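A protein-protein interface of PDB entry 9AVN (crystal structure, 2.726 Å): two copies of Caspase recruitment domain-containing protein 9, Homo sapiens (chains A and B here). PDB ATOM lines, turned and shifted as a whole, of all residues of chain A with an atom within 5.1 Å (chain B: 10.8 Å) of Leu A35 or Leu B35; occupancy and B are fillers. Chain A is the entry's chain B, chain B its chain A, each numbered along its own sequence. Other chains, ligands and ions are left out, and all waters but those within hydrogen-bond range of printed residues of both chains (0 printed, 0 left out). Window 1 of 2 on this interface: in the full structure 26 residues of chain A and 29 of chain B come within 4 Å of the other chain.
The side-chain hydroxyl (OG) of Ser A39 sits at hydrogen-bond distance from the side-chain amide nitrogen (NE2) of Gln B38, 2.9 Å away.
The side-chain amide nitrogen of Gln A38 is in hydrogen-bond range of the side-chain hydroxyl of Ser B39, 3.3 Å away.
NZ of Lys B42 lies close to NE2 of Gln A38, 3.4 Å away.
The side-chain carboxylate (OD2) of Asp B30 lies within salt-bridge range of the guanidinium group (NH1) of Arg B34 (3.3 Å).
O of Leu B35 sits at hydrogen-bond distance from OG of Ser B39 (3.1 Å).
The side-chain hydroxyl (OG) of Ser A39 is in hydrogen-bond range of the backbone carbonyl oxygen (O) of Leu A35 (3.1 Å).
A ring nitrogen (ND1) of His A37 is in hydrogen-bond range of the side-chain amide oxygen (OE1) of Gln A38.
Asn B28 touches Leu A31.
Leu A31 touches Leu B31 (CB to CB, 3.9 Å).
CD2 of Leu A31 touches CD2 of Leu B35 (3.7 Å).
Leu B35 touches Arg A34 (CD2 to CZ, 3.4 Å).
Leu A35 touches Arg B34.
Leu B35 touches Leu A35 (N to CD1, 3.7 Å).
Gln B38 touches Leu A35 (CG to CD1, 3.4 Å).
CG of Gln A38 touches CD1 of Leu B35 (3.8 Å).
Gln A38 touches Gln B38.
Leu A31 touches three residues of chain B.
No residue of chain B comes within 4 Å of Ala A32.
Printed residues of chain B within 4 Å of Leu A35: Arg B34, Leu B35 and Gln B38.
Gln A38 touches just these residues of chain B: Leu B35 (3.8 Å), Gln B38 (3.9 Å), Ser B39 (3.3 Å) and Lys B42 (3.4 Å).
Ser A39 touches one residue of chain B.
Printed residues of chain A within 4 Å of Leu B31: Leu A31.
Leu B35 touches four residues of chain A.
Printed residues of chain A within 4 Å of Gln B38: Leu A35, Gln A38 and Ser A39.
Of the printed residues of chain A, Ser B39 touches Gln A38 (3.3 Å).
The nearest printed residue of chain B that does not touch Leu A35 is Leu B31 (4.01 Å).
Hydrophobic or aromatic side chains of chain B that line the printed part of chain A: Leu B31 and Leu B35.
Among the printed residues, 12 pairs touch across the chains.
Among the printed residues, no Asp or Glu carboxylate lies within 4 Å of a Lys or Arg side-chain nitrogen of the other chain.
Leu A31 touches its own counterpart, Leu B31.
Leu B35 touches its own counterpart, Leu A35.
Leu A35 touches Gln B38, and with the chains exchanged Gln A38 touches Leu B35.
Gln B38 touches its own counterpart, Gln A38.
10 positions are printed for both chains.
Of the 12 pairs that touch across the chains among the printed residues, 9 have their exchanged pair printed and touching as well.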
ATOM      1  N   ASP A  30       0.230  -1.506  16.721  1.00  0.00           N
ATOM      2  CA  ASP A  30       1.241  -1.537  17.780  1.00  0.00           C
ATOM      3  C   ASP A  30       0.919  -2.602  18.835  1.00  0.00           C
ATOM      4  O   ASP A  30       1.814  -3.338  19.271  1.00  0.00           O
ATOM      5  CB  ASP A  30       1.413  -0.151  18.414  1.00  0.00           C
ATOM      6  CG  ASP A  30       2.005   0.890  17.464  1.00  0.00           C
ATOM      7  OD1 ASP A  30       1.864   2.116  17.748  1.00  0.00           O
ATOM      8  OD2 ASP A  30       2.587   0.486  16.422  1.00  0.00           O
ATOM      9  N   LEU A  31      -0.361  -2.724  19.218  1.00  0.00           N
ATOM     10  CA  LEU A  31      -0.771  -3.739  20.189  1.00  0.00           C
ATOM     11  C   LEU A  31      -0.572  -5.154  19.595  1.00  0.00           C
ATOM     12  O   LEU A  31      -0.170  -6.051  20.312  1.00  0.00           O
ATOM     13  CB  LEU A  31      -2.237  -3.539  20.612  1.00  0.00           C
ATOM     14  CG  LEU A  31      -2.519  -2.379  21.555  1.00  0.00           C
ATOM     15  CD1 LEU A  31      -4.013  -2.151  21.720  1.00  0.00           C
ATOM     16  CD2 LEU A  31      -1.855  -2.611  22.897  1.00  0.00           C
ATOM     17  N   ALA A  32      -0.836  -5.344  18.297  1.00  0.00           N
ATOM     18  CA  ALA A  32      -0.617  -6.630  17.626  1.00  0.00           C
ATOM     19  C   ALA A  32       0.871  -6.988  17.587  1.00  0.00           C
ATOM     20  O   ALA A  32       1.206  -8.153  17.771  1.00  0.00           O
ATOM     21  CB  ALA A  32      -1.154  -6.602  16.211  1.00  0.00           C
ATOM     22  N   MET A  33       1.751  -6.001  17.356  1.00  0.00           N
ATOM     23  CA  MET A  33       3.179  -6.235  17.339  1.00  0.00           C
ATOM     24  C   MET A  33       3.686  -6.591  18.728  1.00  0.00           C
ATOM     25  O   MET A  33       4.533  -7.474  18.871  1.00  0.00           O
ATOM     26  CB  MET A  33       3.902  -4.993  16.810  1.00  0.00           C
ATOM     27  CG  MET A  33       3.667  -4.734  15.325  1.00  0.00           C
ATOM     28  SD  MET A  33       3.918  -6.176  14.230  1.00  0.00           S
ATOM     29  CE  MET A  33       2.365  -6.317  13.556  1.00  0.00           C
ATOM     30  N   ARG A  34       3.167  -5.918  19.758  1.00  0.00           N
ATOM     31  CA  ARG A  34       3.543  -6.215  21.130  1.00  0.00           C
ATOM     32  C   ARG A  34       3.034  -7.588  21.558  1.00  0.00           C
ATOM     33  O   ARG A  34       3.755  -8.329  22.220  1.00  0.00           O
ATOM     34  CB  ARG A  34       3.023  -5.127  22.059  1.00  0.00           C
ATOM     35  CG  ARG A  34       3.790  -3.811  21.895  1.00  0.00           C
ATOM     36  CD  ARG A  34       3.100  -2.666  22.563  1.00  0.00           C
ATOM     37  NE  ARG A  34       3.064  -2.858  24.010  1.00  0.00           N
ATOM     38  CZ  ARG A  34       2.176  -2.288  24.824  1.00  0.00           C
ATOM     39  NH1 ARG A  34       1.238  -1.471  24.334  1.00  0.00           N
ATOM     40  NH2 ARG A  34       2.203  -2.545  26.133  1.00  0.00           N
ATOM     41  N   LEU A  35       1.834  -7.952  21.147  1.00  0.00           N
ATOM     42  CA  LEU A  35       1.262  -9.257  21.445  1.00  0.00           C
ATOM     43  C   LEU A  35       2.075 -10.378  20.767  1.00  0.00           C
ATOM     44  O   LEU A  35       2.307 -11.428  21.378  1.00  0.00           O
ATOM     45  CB  LEU A  35      -0.199  -9.272  20.978  1.00  0.00           C
ATOM     46  CG  LEU A  35      -1.008 -10.528  21.095  1.00  0.00           C
ATOM     47  CD1 LEU A  35      -1.071 -10.973  22.495  1.00  0.00           C
ATOM     48  CD2 LEU A  35      -2.418 -10.263  20.584  1.00  0.00           C
ATOM     49  N   ALA A  36       2.545 -10.142  19.526  1.00  0.00           N
ATOM     50  CA  ALA A  36       3.352 -11.125  18.816  1.00  0.00           C
ATOM     51  C   ALA A  36       4.713 -11.267  19.500  1.00  0.00           C
ATOM     52  O   ALA A  36       5.213 -12.386  19.630  1.00  0.00           O
ATOM     53  CB  ALA A  36       3.517 -10.729  17.370  1.00  0.00           C
ATOM     54  N   HIS A  37       5.269 -10.162  20.005  1.00  0.00           N
ATOM     55  CA  HIS A  37       6.532 -10.173  20.724  1.00  0.00           C
ATOM     56  C   HIS A  37       6.447 -10.997  21.994  1.00  0.00           C
ATOM     57  O   HIS A  37       7.314 -11.843  22.239  1.00  0.00           O
ATOM     58  CB  HIS A  37       6.940  -8.741  21.090  1.00  0.00           C
ATOM     59  CG  HIS A  37       8.245  -8.679  21.805  1.00  0.00           C
ATOM     60  ND1 HIS A  37       8.317  -8.798  23.183  1.00  0.00           N
ATOM     61  CD2 HIS A  37       9.498  -8.558  21.305  1.00  0.00           C
ATOM     62  CE1 HIS A  37       9.603  -8.717  23.479  1.00  0.00           C
ATOM     63  NE2 HIS A  37      10.352  -8.580  22.378  1.00  0.00           N
ATOM     64  N   GLN A  38       5.405 -10.758  22.810  1.00  0.00           N
ATOM     65  CA  GLN A  38       5.244 -11.478  24.068  1.00  0.00           C
ATOM     66  C   GLN A  38       4.991 -12.963  23.831  1.00  0.00           C
ATOM     67  O   GLN A  38       5.461 -13.791  24.605  1.00  0.00           O
ATOM     68  CB  GLN A  38       4.136 -10.842  24.919  1.00  0.00           C
ATOM     69  CG  GLN A  38       4.429  -9.402  25.318  1.00  0.00           C
ATOM     70  CD  GLN A  38       5.553  -9.303  26.308  1.00  0.00           C
ATOM     71  OE1 GLN A  38       6.588  -8.684  26.052  1.00  0.00           O
ATOM     72  NE2 GLN A  38       5.368  -9.888  27.475  1.00  0.00           N
ATOM     73  N   SER A  39       4.276 -13.313  22.744  1.00  0.00           N
ATOM     74  CA  SER A  39       4.030 -14.707  22.416  1.00  0.00           C
ATOM     75  C   SER A  39       5.326 -15.418  22.031  1.00  0.00           C
ATOM     76  O   SER A  39       5.499 -16.585  22.362  1.00  0.00           O
ATOM     77  CB  SER A  39       3.016 -14.804  21.294  1.00  0.00           C
ATOM     78  OG  SER A  39       1.723 -14.433  21.733  1.00  0.00           O
ATOM     79  N   GLU B  27     -11.817  -4.047  18.838  1.00  0.00           N
ATOM     80  CA  GLU B  27     -10.631  -4.821  18.525  1.00  0.00           C
ATOM     81  C   GLU B  27      -9.487  -4.380  19.428  1.00  0.00           C
ATOM     82  O   GLU B  27      -8.768  -5.221  19.935  1.00  0.00           O
ATOM     83  CB  GLU B  27     -10.189  -4.627  17.074  1.00  0.00           C
ATOM     84  CG  GLU B  27     -11.064  -5.259  16.024  1.00  0.00           C
ATOM     85  CD  GLU B  27     -10.503  -5.106  14.615  1.00  0.00           C
ATOM     86  OE1 GLU B  27     -11.263  -4.690  13.708  1.00  0.00           O
ATOM     87  OE2 GLU B  27      -9.303  -5.405  14.414  1.00  0.00           O
ATOM     88  N   ASN B  28      -9.322  -3.070  19.629  1.00  0.00           N
ATOM     89  CA  ASN B  28      -8.291  -2.487  20.470  1.00  0.00           C
ATOM     90  C   ASN B  28      -8.388  -3.010  21.896  1.00  0.00           C
ATOM     91  O   ASN B  28      -7.374  -3.418  22.467  1.00  0.00           O
ATOM     92  CB  ASN B  28      -8.450  -0.963  20.432  1.00  0.00           C
ATOM     93  CG  ASN B  28      -7.421  -0.169  21.153  1.00  0.00           C
ATOM     94  OD1 ASN B  28      -6.354   0.110  20.604  1.00  0.00           O
ATOM     95  ND2 ASN B  28      -7.732   0.269  22.373  1.00  0.00           N
ATOM     96  N   TYR B  29      -9.611  -3.046  22.452  1.00  0.00           N
ATOM     97  CA  TYR B  29      -9.813  -3.566  23.797  1.00  0.00           C
ATOM     98  C   TYR B  29      -9.415  -5.048  23.886  1.00  0.00           C
ATOM     99  O   TYR B  29      -8.719  -5.440  24.822  1.00  0.00           O
ATOM    100  CB  TYR B  29     -11.267  -3.368  24.237  1.00  0.00           C
ATOM    101  CG  TYR B  29     -11.500  -3.784  25.672  1.00  0.00           C
ATOM    102  CD1 TYR B  29     -11.249  -2.910  26.723  1.00  0.00           C
ATOM    103  CD2 TYR B  29     -11.951  -5.059  25.983  1.00  0.00           C
ATOM    104  CE1 TYR B  29     -11.462  -3.288  28.051  1.00  0.00           C
ATOM    105  CE2 TYR B  29     -12.170  -5.450  27.307  1.00  0.00           C
ATOM    106  CZ  TYR B  29     -11.931  -4.560  28.341  1.00  0.00           C
ATOM    107  OH  TYR B  29     -12.132  -4.944  29.656  1.00  0.00           O
ATOM    108  N   ASP B  30      -9.815  -5.853  22.893  1.00  0.00           N
ATOM    109  CA  ASP B  30      -9.484  -7.275  22.835  1.00  0.00           C
ATOM    110  C   ASP B  30      -7.996  -7.492  22.696  1.00  0.00           C
ATOM    111  O   ASP B  30      -7.471  -8.354  23.375  1.00  0.00           O
ATOM    112  CB  ASP B  30     -10.288  -7.982  21.722  1.00  0.00           C
ATOM    113  CG  ASP B  30      -9.738  -9.290  21.105  1.00  0.00           C
ATOM    114  OD1 ASP B  30     -10.176 -10.391  21.532  1.00  0.00           O
ATOM    115  OD2 ASP B  30      -8.934  -9.210  20.142  1.00  0.00           O
ATOM    116  N   LEU B  31      -7.301  -6.689  21.880  1.00  0.00           N
ATOM    117  CA  LEU B  31      -5.843  -6.797  21.712  1.00  0.00           C
ATOM    118  C   LEU B  31      -5.130  -6.450  23.009  1.00  0.00           C
ATOM    119  O   LEU B  31      -4.130  -7.095  23.349  1.00  0.00           O
ATOM    120  CB  LEU B  31      -5.322  -5.910  20.583  1.00  0.00           C
ATOM    121  CG  LEU B  31      -5.605  -6.374  19.159  1.00  0.00           C
ATOM    122  CD1 LEU B  31      -5.256  -5.297  18.141  1.00  0.00           C
ATOM    123  CD2 LEU B  31      -4.835  -7.576  18.840  1.00  0.00           C
ATOM    124  N   ALA B  32      -5.651  -5.466  23.760  1.00  0.00           N
ATOM    125  CA  ALA B  32      -5.038  -5.083  25.034  1.00  0.00           C
ATOM    126  C   ALA B  32      -5.193  -6.207  26.062  1.00  0.00           C
ATOM    127  O   ALA B  32      -4.263  -6.486  26.830  1.00  0.00           O
ATOM    128  CB  ALA B  32      -5.671  -3.798  25.556  1.00  0.00           C
ATOM    129  N   MET B  33      -6.358  -6.864  26.064  1.00  0.00           N
ATOM    130  CA  MET B  33      -6.600  -7.966  26.968  1.00  0.00           C
ATOM    131  C   MET B  33      -5.741  -9.171  26.641  1.00  0.00           C
ATOM    132  O   MET B  33      -5.249  -9.833  27.564  1.00  0.00           O
ATOM    133  CB  MET B  33      -8.068  -8.329  26.971  1.00  0.00           C
ATOM    134  CG  MET B  33      -8.923  -7.252  27.583  1.00  0.00           C
ATOM    135  SD  MET B  33      -8.330  -6.533  29.175  1.00  0.00           S
ATOM    136  CE  MET B  33      -8.118  -4.856  28.718  1.00  0.00           C
ATOM    137  N   ARG B  34      -5.549  -9.452  25.327  1.00  0.00           N
ATOM    138  CA  ARG B  34      -4.704 -10.543  24.868  1.00  0.00           C
ATOM    139  C   ARG B  34      -3.236 -10.260  25.209  1.00  0.00           C
ATOM    140  O   ARG B  34      -2.522 -11.163  25.635  1.00  0.00           O
ATOM    141  CB  ARG B  34      -4.907 -10.751  23.379  1.00  0.00           C
ATOM    142  CG  ARG B  34      -6.235 -11.437  23.069  1.00  0.00           C
ATOM    143  CD  ARG B  34      -6.609 -11.304  21.606  1.00  0.00           C
ATOM    144  NE  ARG B  34      -5.682 -12.003  20.721  1.00  0.00           N
ATOM    145  CZ  ARG B  34      -5.618 -11.828  19.403  1.00  0.00           C
ATOM    146  NH1 ARG B  34      -6.402 -10.942  18.806  1.00  0.00           N
ATOM    147  NH2 ARG B  34      -4.767 -12.544  18.669  1.00  0.00           N
ATOM    148  N   LEU B  35      -2.800  -8.999  25.095  1.00  0.00           N
ATOM    149  CA  LEU B  35      -1.448  -8.587  25.450  1.00  0.00           C
ATOM    150  C   LEU B  35      -1.193  -8.768  26.956  1.00  0.00           C
ATOM    151  O   LEU B  35      -0.110  -9.219  27.345  1.00  0.00           O
ATOM    152  CB  LEU B  35      -1.255  -7.132  25.021  1.00  0.00           C
ATOM    153  CG  LEU B  35       0.109  -6.484  25.301  1.00  0.00           C
ATOM    154  CD1 LEU B  35       1.287  -7.324  24.772  1.00  0.00           C
ATOM    155  CD2 LEU B  35       0.134  -5.048  24.754  1.00  0.00           C
ATOM    156  N   ALA B  36      -2.206  -8.469  27.810  1.00  0.00           N
ATOM    157  CA  ALA B  36      -2.101  -8.675  29.264  1.00  0.00           C
ATOM    158  C   ALA B  36      -2.017 -10.172  29.593  1.00  0.00           C
ATOM    159  O   ALA B  36      -1.246 -10.565  30.454  1.00  0.00           O
ATOM    160  CB  ALA B  36      -3.286  -8.061  29.975  1.00  0.00           C
ATOM    161  N   HIS B  37      -2.774 -11.010  28.884  1.00  0.00           N
ATOM    162  CA  HIS B  37      -2.738 -12.448  29.098  1.00  0.00           C
ATOM    163  C   HIS B  37      -1.374 -13.026  28.718  1.00  0.00           C
ATOM    164  O   HIS B  37      -0.866 -13.884  29.445  1.00  0.00           O
ATOM    165  CB  HIS B  37      -3.900 -13.154  28.376  1.00  0.00           C
ATOM    166  CG  HIS B  37      -3.771 -14.647  28.302  1.00  0.00           C
ATOM    167  ND1 HIS B  37      -4.100 -15.464  29.378  1.00  0.00           N
ATOM    168  CD2 HIS B  37      -3.312 -15.419  27.284  1.00  0.00           C
ATOM    169  CE1 HIS B  37      -3.837 -16.696  28.974  1.00  0.00           C
ATOM    170  NE2 HIS B  37      -3.359 -16.715  27.717  1.00  0.00           N
ATOM    171  N   GLN B  38      -0.790 -12.584  27.590  1.00  0.00           N
ATOM    172  CA  GLN B  38       0.516 -13.095  27.182  1.00  0.00           C
ATOM    173  C   GLN B  38       1.617 -12.635  28.136  1.00  0.00           C
ATOM    174  O   GLN B  38       2.540 -13.388  28.392  1.00  0.00           O
ATOM    175  CB  GLN B  38       0.840 -12.754  25.717  1.00  0.00           C
ATOM    176  CG  GLN B  38      -0.133 -13.393  24.723  1.00  0.00           C
ATOM    177  CD  GLN B  38      -0.040 -14.899  24.639  1.00  0.00           C
ATOM    178  OE1 GLN B  38      -1.027 -15.615  24.842  1.00  0.00           O
ATOM    179  NE2 GLN B  38       1.137 -15.430  24.348  1.00  0.00           N
ATOM    180  N   SER B  39       1.495 -11.439  28.713  1.00  0.00           N
ATOM    181  CA  SER B  39       2.458 -10.955  29.696  1.00  0.00           C
ATOM    182  C   SER B  39       2.404 -11.787  30.985  1.00  0.00           C
ATOM    183  O   SER B  39       3.438 -12.067  31.577  1.00  0.00           O
ATOM    184  CB  SER B  39       2.210  -9.480  29.990  1.00  0.00           C
ATOM    185  OG  SER B  39       2.584  -8.680  28.873  1.00  0.00           O
ATOM    186  N   GLU B  40       1.211 -12.221  31.396  1.00  0.00           N
ATOM    187  CA  GLU B  40       1.054 -13.088  32.564  1.00  0.00           C
ATOM    188  C   GLU B  40       1.665 -14.488  32.290  1.00  0.00           C
ATOM    189  O   GLU B  40       2.315 -15.065  33.146  1.00  0.00           O
ATOM    190  CB  GLU B  40      -0.430 -13.281  32.897  1.00  0.00           C
ATOM    191  CG  GLU B  40      -1.145 -12.109  33.518  1.00  0.00           C
ATOM    192  CD  GLU B  40      -2.653 -12.300  33.590  1.00  0.00           C
ATOM    193  OE1 GLU B  40      -3.382 -11.280  33.584  1.00  0.00           O
ATOM    194  OE2 GLU B  40      -3.114 -13.464  33.595  1.00  0.00           O
ATOM    195  N   GLU B  41       1.404 -15.041  31.111  1.00  0.00           N
ATOM    196  CA  GLU B  41       1.915 -16.335  30.714  1.00  0.00           C
ATOM    197  C   GLU B  41       3.437 -16.313  30.574  1.00  0.00           C
ATOM    198  O   GLU B  41       4.095 -17.304  30.895  1.00  0.00           O
ATOM    199  CB  GLU B  41       1.304 -16.742  29.387  1.00  0.00           C
ATOM    200  CG  GLU B  41      -0.150 -17.133  29.444  1.00  0.00           C
ATOM    201  CD  GLU B  41      -0.336 -18.399  28.655  1.00  0.00           C
ATOM    202  OE1 GLU B  41       0.219 -19.436  29.088  1.00  0.00           O
ATOM    203  OE2 GLU B  41      -0.994 -18.351  27.590  1.00  0.00           O
ATOM    204  N   LYS B  42       3.994 -15.200  30.083  1.00  0.00           N
ATOM    205  CA  LYS B  42       5.438 -15.036  29.951  1.00  0.00           C
ATOM    206  C   LYS B  42       6.061 -14.929  31.339  1.00  0.00           C
ATOM    207  O   LYS B  42       7.035 -15.621  31.611  1.00  0.00           O
ATOM    208  CB  LYS B  42       5.790 -13.775  29.138  1.00  0.00           C
ATOM    209  CG  LYS B  42       7.259 -13.681  28.832  1.00  0.00           C
ATOM    210  CD  LYS B  42       7.648 -12.303  28.366  1.00  0.00           C
ATOM    211  CE  LYS B  42       7.870 -11.378  29.529  1.00  0.00           C
ATOM    212  NZ  LYS B  42       8.380 -10.058  29.080  1.00  0.00           N
ATOM    213  N   GLY B  43       5.475 -14.099  32.206  1.00  0.00           N
ATOM    214  CA  GLY B  43       5.938 -13.922  33.574  1.00  0.00           C
ATOM    215  C   GLY B  43       5.971 -15.220  34.352  1.00  0.00           C
ATOM    216  O   GLY B  43       6.933 -15.477  35.072  1.00  0.00           O
